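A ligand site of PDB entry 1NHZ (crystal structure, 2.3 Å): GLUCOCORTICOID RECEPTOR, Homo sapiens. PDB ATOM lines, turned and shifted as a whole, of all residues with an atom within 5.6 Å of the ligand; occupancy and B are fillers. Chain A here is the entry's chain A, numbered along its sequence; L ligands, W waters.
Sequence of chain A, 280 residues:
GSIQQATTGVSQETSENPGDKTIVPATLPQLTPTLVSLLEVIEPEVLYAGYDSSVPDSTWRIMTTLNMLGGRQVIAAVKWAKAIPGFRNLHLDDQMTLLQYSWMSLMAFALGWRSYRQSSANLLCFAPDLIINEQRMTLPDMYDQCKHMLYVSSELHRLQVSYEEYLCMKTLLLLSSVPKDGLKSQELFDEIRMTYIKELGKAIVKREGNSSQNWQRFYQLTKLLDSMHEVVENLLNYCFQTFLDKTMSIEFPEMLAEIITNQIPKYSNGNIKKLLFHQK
NE2 of Gln 145 is in hydrogen-bond range of O2 of the ligand, 2.7 Å away.
An oxygen (O1) of the ligand sits close to the side-chain amide oxygen of Gln 73 (2.8 Å).
An oxygen (O1) of the ligand lies within hydrogen-bond range of the guanidinium group of Arg 114, at 2.8 Å.
The side-chain amide oxygen (OE1) of Gln 145 sits close to the side-chain sulfur (SD) of Met 63 (3.8 Å).
The guanidinium group (NH2) of Arg 114 lies within hydrogen-bond range of the backbone carbonyl oxygen (O) of Phe 126 (2.8 Å).
NE of Arg 114 is in hydrogen-bond range of O of Cys 125, 3.2 Å away.
The backbone NH (N) of Val 74 lies close to the side-chain sulfur (SD) of Met 107, 3.7 Å away.
CE of Met 63 touches O2 of the ligand, at 3.6 Å.
O of Leu 66 touches C17 of the ligand, at 3.2 Å.
CA of Asn 67 touches C17 of the ligand (3.8 Å).
Gly 70 touches the ligand.
Val 74 touches the ligand.
Trp 103 touches the ligand (CZ3 to C12, 3.7 Å).
Met 104 touches the ligand (SD to C29, 3.6 Å).
Met 107 touches the ligand (CB to C5, 3.6 Å).
N of Ala 108 touches C5 of the ligand, at 3.8 Å.
CD2 of Leu 111 touches C3 of the ligand, at 3.7 Å.
Phe 126 touches the ligand.
Met 149 touches the ligand.
Leu 235 touches the ligand (CD2 to C26, 3.6 Å).
Tyr 238 touches the ligand (CB to O2, 3.98 Å).
Phe 240 touches the ligand (CE1 to C14, 3.7 Å).
Hydrophobic or aromatic side chains within 4 Å of the ligand: Met 63, Leu 66, Val 74, Trp 103, Met 104, Met 107, Leu 111, Phe 126, Met 149, Leu 235, Tyr 238 and Phe 240.
Within 4 Å of the ligand: Met 63, Leu 66, Asn 67, Gly 70, Gln 73, Val 74, Trp 103, Met 104, Met 107, Ala 108, Leu 111, Arg 114, Phe 126, Gln 145, Met 149, Leu 235, Tyr 238 and Phe 240.
Water W1 bridges an oxygen (O2) of the ligand and the backbone carbonyl oxygen of Cys 239.
Water W2 lies within hydrogen-bond range of the backbone carbonyl oxygen (O) of Met 107, the side-chain amide nitrogen (NE2) of Gln 73, the guanidinium group (NH1) of Arg 114 and an oxygen (O1) of the ligand.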
ATOM      1  N   MET A  63     -15.399 -17.656 -32.861  1.00  0.00           N
ATOM      2  CA  MET A  63     -14.010 -17.960 -32.472  1.00  0.00           C
ATOM      3  C   MET A  63     -13.002 -17.253 -33.368  1.00  0.00           C
ATOM      4  O   MET A  63     -11.923 -16.806 -32.939  1.00  0.00           O
ATOM      5  CB  MET A  63     -13.774 -19.469 -32.519  1.00  0.00           C
ATOM      6  CG  MET A  63     -14.579 -20.246 -31.508  1.00  0.00           C
ATOM      7  SD  MET A  63     -14.519 -19.605 -29.770  1.00  0.00           S
ATOM      8  CE  MET A  63     -12.701 -19.686 -29.461  1.00  0.00           C
ATOM      9  N   LEU A  66     -13.085 -13.731 -32.304  1.00  0.00           N
ATOM     10  CA  LEU A  66     -12.393 -13.608 -31.014  1.00  0.00           C
ATOM     11  C   LEU A  66     -10.881 -13.707 -31.159  1.00  0.00           C
ATOM     12  O   LEU A  66     -10.127 -13.185 -30.323  1.00  0.00           O
ATOM     13  CB  LEU A  66     -12.900 -14.642 -30.009  1.00  0.00           C
ATOM     14  CG  LEU A  66     -14.161 -14.275 -29.230  1.00  0.00           C
ATOM     15  CD1 LEU A  66     -14.576 -15.462 -28.377  1.00  0.00           C
ATOM     16  CD2 LEU A  66     -13.911 -13.084 -28.334  1.00  0.00           C
ATOM     17  N   ASN A  67     -10.433 -14.402 -32.194  1.00  0.00           N
ATOM     18  CA  ASN A  67      -9.009 -14.494 -32.496  1.00  0.00           C
ATOM     19  C   ASN A  67      -8.464 -13.145 -32.831  1.00  0.00           C
ATOM     20  O   ASN A  67      -7.464 -12.738 -32.290  1.00  0.00           O
ATOM     21  CB  ASN A  67      -8.711 -15.442 -33.658  1.00  0.00           C
ATOM     22  CG  ASN A  67      -7.250 -15.834 -33.698  1.00  0.00           C
ATOM     23  OD1 ASN A  67      -6.461 -15.220 -34.408  1.00  0.00           O
ATOM     24  ND2 ASN A  67      -6.879 -16.787 -32.859  1.00  0.00           N
ATOM     25  N   LEU A  69      -9.969 -10.138 -32.187  1.00  0.00           N
ATOM     26  CA  LEU A  69     -10.105  -9.266 -31.047  1.00  0.00           C
ATOM     27  C   LEU A  69      -9.030  -9.574 -29.989  1.00  0.00           C
ATOM     28  O   LEU A  69      -8.489  -8.666 -29.378  1.00  0.00           O
ATOM     29  CB  LEU A  69     -11.530  -9.371 -30.461  1.00  0.00           C
ATOM     30  CG  LEU A  69     -11.769  -8.617 -29.140  1.00  0.00           C
ATOM     31  CD1 LEU A  69     -11.642  -7.107 -29.368  1.00  0.00           C
ATOM     32  CD2 LEU A  69     -13.089  -8.974 -28.579  1.00  0.00           C
ATOM     33  N   GLY A  70      -8.733 -10.844 -29.734  1.00  0.00           N
ATOM     34  CA  GLY A  70      -7.722 -11.220 -28.750  1.00  0.00           C
ATOM     35  C   GLY A  70      -6.300 -10.734 -29.036  1.00  0.00           C
ATOM     36  O   GLY A  70      -5.576 -10.279 -28.132  1.00  0.00           O
ATOM     37  N   GLY A  71      -5.902 -10.808 -30.304  1.00  0.00           N
ATOM     38  CA  GLY A  71      -4.661 -10.203 -30.740  1.00  0.00           C
ATOM     39  C   GLY A  71      -4.662  -8.724 -30.452  1.00  0.00           C
ATOM     40  O   GLY A  71      -3.681  -8.187 -29.896  1.00  0.00           O
ATOM     41  N   GLN A  73      -6.328  -7.084 -28.185  1.00  0.00           N
ATOM     42  CA  GLN A  73      -6.352  -6.831 -26.741  1.00  0.00           C
ATOM     43  C   GLN A  73      -4.974  -7.034 -26.123  1.00  0.00           C
ATOM     44  O   GLN A  73      -4.594  -6.269 -25.244  1.00  0.00           O
ATOM     45  CB  GLN A  73      -7.373  -7.730 -26.040  1.00  0.00           C
ATOM     46  CG  GLN A  73      -8.822  -7.364 -26.302  1.00  0.00           C
ATOM     47  CD  GLN A  73      -9.830  -7.988 -25.313  1.00  0.00           C
ATOM     48  OE1 GLN A  73     -11.036  -7.684 -25.372  1.00  0.00           O
ATOM     49  NE2 GLN A  73      -9.366  -8.836 -24.434  1.00  0.00           N
ATOM     50  N   VAL A  74      -4.229  -8.039 -26.603  1.00  0.00           N
ATOM     51  CA  VAL A  74      -2.825  -8.242 -26.264  1.00  0.00           C
ATOM     52  C   VAL A  74      -2.003  -6.997 -26.589  1.00  0.00           C
ATOM     53  O   VAL A  74      -1.265  -6.533 -25.754  1.00  0.00           O
ATOM     54  CB  VAL A  74      -2.226  -9.481 -26.956  1.00  0.00           C
ATOM     55  CG1 VAL A  74      -0.704  -9.607 -26.728  1.00  0.00           C
ATOM     56  CG2 VAL A  74      -2.832 -10.712 -26.417  1.00  0.00           C
ATOM     57  N   TRP A 103      -0.526 -12.149 -19.727  1.00  0.00           N
ATOM     58  CA  TRP A 103      -1.530 -11.566 -20.649  1.00  0.00           C
ATOM     59  C   TRP A 103      -2.915 -12.241 -20.637  1.00  0.00           C
ATOM     60  O   TRP A 103      -3.938 -11.578 -20.730  1.00  0.00           O
ATOM     61  CB  TRP A 103      -1.002 -11.415 -22.086  1.00  0.00           C
ATOM     62  CG  TRP A 103      -0.779 -12.667 -22.833  1.00  0.00           C
ATOM     63  CD1 TRP A 103       0.415 -13.269 -23.051  1.00  0.00           C
ATOM     64  CD2 TRP A 103      -1.770 -13.474 -23.503  1.00  0.00           C
ATOM     65  NE1 TRP A 103       0.247 -14.400 -23.810  1.00  0.00           N
ATOM     66  CE2 TRP A 103      -1.083 -14.556 -24.106  1.00  0.00           C
ATOM     67  CE3 TRP A 103      -3.147 -13.400 -23.677  1.00  0.00           C
ATOM     68  CZ2 TRP A 103      -1.738 -15.550 -24.853  1.00  0.00           C
ATOM     69  CZ3 TRP A 103      -3.805 -14.386 -24.418  1.00  0.00           C
ATOM     70  CH2 TRP A 103      -3.108 -15.437 -25.006  1.00  0.00           C
ATOM     71  N   MET A 104      -2.957 -13.548 -20.473  1.00  0.00           N
ATOM     72  CA  MET A 104      -4.264 -14.206 -20.483  1.00  0.00           C
ATOM     73  C   MET A 104      -5.017 -13.825 -19.195  1.00  0.00           C
ATOM     74  O   MET A 104      -6.195 -13.557 -19.214  1.00  0.00           O
ATOM     75  CB  MET A 104      -4.118 -15.709 -20.605  1.00  0.00           C
ATOM     76  CG  MET A 104      -5.427 -16.524 -20.635  1.00  0.00           C
ATOM     77  SD  MET A 104      -6.377 -16.234 -22.186  1.00  0.00           S
ATOM     78  CE  MET A 104      -5.704 -17.582 -23.201  1.00  0.00           C
ATOM     79  N   MET A 107      -6.438 -10.226 -19.501  1.00  0.00           N
ATOM     80  CA  MET A 107      -7.598 -10.168 -20.405  1.00  0.00           C
ATOM     81  C   MET A 107      -8.839 -10.848 -19.845  1.00  0.00           C
ATOM     82  O   MET A 107      -9.952 -10.344 -20.041  1.00  0.00           O
ATOM     83  CB  MET A 107      -7.222 -10.744 -21.771  1.00  0.00           C
ATOM     84  CG  MET A 107      -6.357  -9.727 -22.531  1.00  0.00           C
ATOM     85  SD  MET A 107      -5.459 -10.413 -23.992  1.00  0.00           S
ATOM     86  CE  MET A 107      -6.802 -11.285 -24.726  1.00  0.00           C
ATOM     87  N   ALA A 108      -8.669 -11.970 -19.157  1.00  0.00           N
ATOM     88  CA  ALA A 108      -9.812 -12.679 -18.540  1.00  0.00           C
ATOM     89  C   ALA A 108     -10.377 -11.856 -17.369  1.00  0.00           C
ATOM     90  O   ALA A 108     -11.584 -11.838 -17.148  1.00  0.00           O
ATOM     91  CB  ALA A 108      -9.373 -14.088 -18.046  1.00  0.00           C
ATOM     92  N   LEU A 111     -12.172  -8.876 -18.886  1.00  0.00           N
ATOM     93  CA  LEU A 111     -13.419  -9.463 -19.360  1.00  0.00           C
ATOM     94  C   LEU A 111     -14.394  -9.648 -18.175  1.00  0.00           C
ATOM     95  O   LEU A 111     -15.570  -9.343 -18.303  1.00  0.00           O
ATOM     96  CB  LEU A 111     -13.178 -10.754 -20.116  1.00  0.00           C
ATOM     97  CG  LEU A 111     -14.343 -11.633 -20.561  1.00  0.00           C
ATOM     98  CD1 LEU A 111     -15.258 -10.923 -21.505  1.00  0.00           C
ATOM     99  CD2 LEU A 111     -13.763 -12.899 -21.245  1.00  0.00           C
ATOM    100  N   ARG A 114     -15.846  -6.229 -17.165  1.00  0.00           N
ATOM    101  CA  ARG A 114     -16.817  -5.787 -18.116  1.00  0.00           C
ATOM    102  C   ARG A 114     -18.131  -6.527 -17.949  1.00  0.00           C
ATOM    103  O   ARG A 114     -19.186  -5.903 -18.023  1.00  0.00           O
ATOM    104  CB  ARG A 114     -16.308  -5.958 -19.577  1.00  0.00           C
ATOM    105  CG  ARG A 114     -15.271  -4.925 -19.964  1.00  0.00           C
ATOM    106  CD  ARG A 114     -14.955  -4.832 -21.448  1.00  0.00           C
ATOM    107  NE  ARG A 114     -14.777  -6.120 -22.073  1.00  0.00           N
ATOM    108  CZ  ARG A 114     -13.639  -6.792 -22.198  1.00  0.00           C
ATOM    109  NH1 ARG A 114     -12.497  -6.368 -21.701  1.00  0.00           N
ATOM    110  NH2 ARG A 114     -13.647  -7.977 -22.794  1.00  0.00           N
ATOM    111  N   CYS A 125     -19.308 -10.488 -21.698  1.00  0.00           N
ATOM    112  CA  CYS A 125     -19.217  -9.309 -22.527  1.00  0.00           C
ATOM    113  C   CYS A 125     -17.820  -9.145 -23.098  1.00  0.00           C
ATOM    114  O   CYS A 125     -17.049  -8.321 -22.633  1.00  0.00           O
ATOM    115  CB  CYS A 125     -19.611  -8.110 -21.689  1.00  0.00           C
ATOM    116  SG  CYS A 125     -21.279  -8.239 -21.058  1.00  0.00           S
ATOM    117  N   PHE A 126     -17.488  -9.919 -24.117  1.00  0.00           N
ATOM    118  CA  PHE A 126     -16.215  -9.749 -24.810  1.00  0.00           C
ATOM    119  C   PHE A 126     -16.011  -8.338 -25.371  1.00  0.00           C
ATOM    120  O   PHE A 126     -14.926  -7.793 -25.332  1.00  0.00           O
ATOM    121  CB  PHE A 126     -16.118 -10.739 -25.937  1.00  0.00           C
ATOM    122  CG  PHE A 126     -15.908 -12.126 -25.480  1.00  0.00           C
ATOM    123  CD1 PHE A 126     -14.833 -12.443 -24.734  1.00  0.00           C
ATOM    124  CD2 PHE A 126     -16.792 -13.136 -25.815  1.00  0.00           C
ATOM    125  CE1 PHE A 126     -14.637 -13.711 -24.312  1.00  0.00           C
ATOM    126  CE2 PHE A 126     -16.579 -14.395 -25.398  1.00  0.00           C
ATOM    127  CZ  PHE A 126     -15.496 -14.684 -24.650  1.00  0.00           C
ATOM    128  N   MET A 142     -19.027 -23.578 -26.605  1.00  0.00           N
ATOM    129  CA  MET A 142     -19.145 -22.290 -25.923  1.00  0.00           C
ATOM    130  C   MET A 142     -19.239 -22.394 -24.403  1.00  0.00           C
ATOM    131  O   MET A 142     -18.493 -21.721 -23.702  1.00  0.00           O
ATOM    132  CB  MET A 142     -20.346 -21.495 -26.423  1.00  0.00           C
ATOM    133  CG  MET A 142     -20.104 -20.761 -27.705  1.00  0.00           C
ATOM    134  SD  MET A 142     -18.703 -19.571 -27.619  1.00  0.00           S
ATOM    135  CE  MET A 142     -18.030 -20.127 -29.052  1.00  0.00           C
ATOM    136  N   GLN A 145     -15.877 -23.381 -22.646  1.00  0.00           N
ATOM    137  CA  GLN A 145     -14.893 -22.316 -22.546  1.00  0.00           C
ATOM    138  C   GLN A 145     -15.386 -21.180 -21.639  1.00  0.00           C
ATOM    139  O   GLN A 145     -14.661 -20.669 -20.753  1.00  0.00           O
ATOM    140  CB  GLN A 145     -14.532 -21.764 -23.933  1.00  0.00           C
ATOM    141  CG  GLN A 145     -13.786 -22.726 -24.850  1.00  0.00           C
ATOM    142  CD  GLN A 145     -13.644 -22.220 -26.286  1.00  0.00           C
ATOM    143  OE1 GLN A 145     -14.635 -22.188 -27.027  1.00  0.00           O
ATOM    144  NE2 GLN A 145     -12.441 -21.803 -26.674  1.00  0.00           N
ATOM    145  N   CYS A 146     -16.636 -20.780 -21.861  1.00  0.00           N
ATOM    146  CA  CYS A 146     -17.194 -19.615 -21.161  1.00  0.00           C
ATOM    147  C   CYS A 146     -17.377 -19.779 -19.668  1.00  0.00           C
ATOM    148  O   CYS A 146     -17.251 -18.837 -18.926  1.00  0.00           O
ATOM    149  CB  CYS A 146     -18.522 -19.221 -21.779  1.00  0.00           C
ATOM    150  SG  CYS A 146     -18.303 -18.577 -23.461  1.00  0.00           S
ATOM    151  N   MET A 149     -14.548 -18.211 -17.643  1.00  0.00           N
ATOM    152  CA  MET A 149     -14.493 -16.732 -17.652  1.00  0.00           C
ATOM    153  C   MET A 149     -15.621 -16.101 -16.846  1.00  0.00           C
ATOM    154  O   MET A 149     -15.489 -15.000 -16.309  1.00  0.00           O
ATOM    155  CB  MET A 149     -14.522 -16.258 -19.102  1.00  0.00           C
ATOM    156  CG  MET A 149     -13.289 -16.811 -19.879  1.00  0.00           C
ATOM    157  SD  MET A 149     -13.202 -16.338 -21.621  1.00  0.00           S
ATOM    158  CE  MET A 149     -13.959 -17.785 -22.348  1.00  0.00           C
ATOM    159  N   LEU A 235      -7.956 -22.115 -19.348  1.00  0.00           N
ATOM    160  CA  LEU A 235      -8.110 -21.363 -20.600  1.00  0.00           C
ATOM    161  C   LEU A 235      -6.981 -21.664 -21.592  1.00  0.00           C
ATOM    162  O   LEU A 235      -7.165 -21.576 -22.803  1.00  0.00           O
ATOM    163  CB  LEU A 235      -8.197 -19.860 -20.326  1.00  0.00           C
ATOM    164  CG  LEU A 235      -9.487 -19.403 -19.617  1.00  0.00           C
ATOM    165  CD1 LEU A 235      -9.455 -17.870 -19.459  1.00  0.00           C
ATOM    166  CD2 LEU A 235     -10.735 -19.850 -20.371  1.00  0.00           C
ATOM    167  N   TYR A 238      -7.229 -24.684 -24.534  1.00  0.00           N
ATOM    168  CA  TYR A 238      -8.020 -24.520 -25.741  1.00  0.00           C
ATOM    169  C   TYR A 238      -7.128 -24.238 -26.962  1.00  0.00           C
ATOM    170  O   TYR A 238      -5.968 -23.861 -26.836  1.00  0.00           O
ATOM    171  CB  TYR A 238      -9.067 -23.426 -25.505  1.00  0.00           C
ATOM    172  CG  TYR A 238     -10.073 -23.882 -24.475  1.00  0.00           C
ATOM    173  CD1 TYR A 238     -10.144 -23.279 -23.228  1.00  0.00           C
ATOM    174  CD2 TYR A 238     -10.912 -24.966 -24.737  1.00  0.00           C
ATOM    175  CE1 TYR A 238     -10.993 -23.696 -22.278  1.00  0.00           C
ATOM    176  CE2 TYR A 238     -11.791 -25.431 -23.774  1.00  0.00           C
ATOM    177  CZ  TYR A 238     -11.835 -24.773 -22.534  1.00  0.00           C
ATOM    178  OH  TYR A 238     -12.702 -25.179 -21.540  1.00  0.00           O
ATOM    179  N   CYS A 239      -7.718 -24.413 -28.133  1.00  0.00           N
ATOM    180  CA  CYS A 239      -7.014 -24.414 -29.413  1.00  0.00           C
ATOM    181  C   CYS A 239      -6.532 -23.034 -29.745  1.00  0.00           C
ATOM    182  O   CYS A 239      -7.324 -22.127 -29.829  1.00  0.00           O
ATOM    183  CB  CYS A 239      -7.942 -24.909 -30.528  1.00  0.00           C
ATOM    184  SG  CYS A 239      -7.221 -24.735 -32.221  1.00  0.00           S
ATOM    185  N   PHE A 240      -5.222 -22.886 -29.946  1.00  0.00           N
ATOM    186  CA  PHE A 240      -4.640 -21.612 -30.337  1.00  0.00           C
ATOM    187  C   PHE A 240      -4.828 -21.353 -31.819  1.00  0.00           C
ATOM    188  O   PHE A 240      -5.118 -20.221 -32.260  1.00  0.00           O
ATOM    189  CB  PHE A 240      -3.143 -21.536 -30.005  1.00  0.00           C
ATOM    190  CG  PHE A 240      -2.473 -20.305 -30.568  1.00  0.00           C
ATOM    191  CD1 PHE A 240      -2.613 -19.055 -29.963  1.00  0.00           C
ATOM    192  CD2 PHE A 240      -1.673 -20.399 -31.699  1.00  0.00           C
ATOM    193  CE1 PHE A 240      -1.974 -17.927 -30.495  1.00  0.00           C
ATOM    194  CE2 PHE A 240      -1.034 -19.271 -32.230  1.00  0.00           C
ATOM    195  CZ  PHE A 240      -1.188 -18.037 -31.628  1.00  0.00           C
HETATM  196  O1  LIG L   1     -12.098  -9.911 -24.111  1.00  0.00           O
HETATM  197  C1  LIG L   1     -11.750 -11.043 -24.258  1.00  0.00           C
HETATM  198  C2  LIG L   1     -12.051 -11.885 -25.562  1.00  0.00           C
HETATM  199  C3  LIG L   1     -10.912 -11.772 -23.242  1.00  0.00           C
HETATM  200  C4  LIG L   1     -10.131 -12.784 -23.682  1.00  0.00           C
HETATM  201  C5  LIG L   1      -9.308 -13.563 -22.596  1.00  0.00           C
HETATM  202  C6  LIG L   1     -10.211 -13.168 -25.124  1.00  0.00           C
HETATM  203  C7  LIG L   1     -10.679 -11.994 -26.122  1.00  0.00           C
HETATM  204  C8  LIG L   1      -9.934 -14.505 -25.441  1.00  0.00           C
HETATM  205  C9  LIG L   1      -9.976 -15.184 -26.948  1.00  0.00           C
HETATM  206  C10 LIG L   1      -8.543 -14.983 -27.582  1.00  0.00           C
HETATM  207  C11 LIG L   1      -7.446 -14.482 -26.760  1.00  0.00           C
HETATM  208  C12 LIG L   1      -6.152 -14.355 -27.215  1.00  0.00           C
HETATM  209  C13 LIG L   1      -5.805 -14.758 -28.560  1.00  0.00           C
HETATM  210  N1  LIG L   1      -4.488 -14.600 -29.140  1.00  0.00           N
HETATM  211  C14 LIG L   1      -4.299 -15.031 -30.530  1.00  0.00           C
HETATM  212  C15 LIG L   1      -3.485 -13.669 -28.582  1.00  0.00           C
HETATM  213  C16 LIG L   1      -6.911 -15.274 -29.400  1.00  0.00           C
HETATM  214  C17 LIG L   1      -8.231 -15.404 -28.918  1.00  0.00           C
HETATM  215  C18 LIG L   1     -10.404 -16.676 -26.878  1.00  0.00           C
HETATM  216  C19 LIG L   1     -10.094 -17.605 -25.657  1.00  0.00           C
HETATM  217  C20 LIG L   1      -8.554 -18.117 -25.925  1.00  0.00           C
HETATM  218  C21 LIG L   1     -10.980 -18.889 -25.585  1.00  0.00           C
HETATM  219  C22 LIG L   1     -12.489 -18.696 -25.566  1.00  0.00           C
HETATM  220  C23 LIG L   1     -13.601 -18.509 -25.979  1.00  0.00           C
HETATM  221  C24 LIG L   1     -15.098 -18.458 -25.979  1.00  0.00           C
HETATM  222  O2  LIG L   1     -10.589 -19.901 -26.552  1.00  0.00           O
HETATM  223  C25 LIG L   1     -10.541 -19.264 -24.138  1.00  0.00           C
HETATM  224  C26 LIG L   1     -10.266 -17.935 -23.365  1.00  0.00           C
HETATM  225  C27 LIG L   1     -10.470 -16.746 -24.388  1.00  0.00           C
HETATM  226  C28 LIG L   1      -9.572 -15.524 -24.203  1.00  0.00           C
HETATM  227  C29 LIG L   1      -9.767 -14.997 -22.722  1.00  0.00           C
HETATM  228  O   HOH W   1      -9.754 -20.115 -29.023  1.00  0.00           O
HETATM  229  O   HOH W   2     -10.341  -8.450 -21.918  1.00  0.00           O
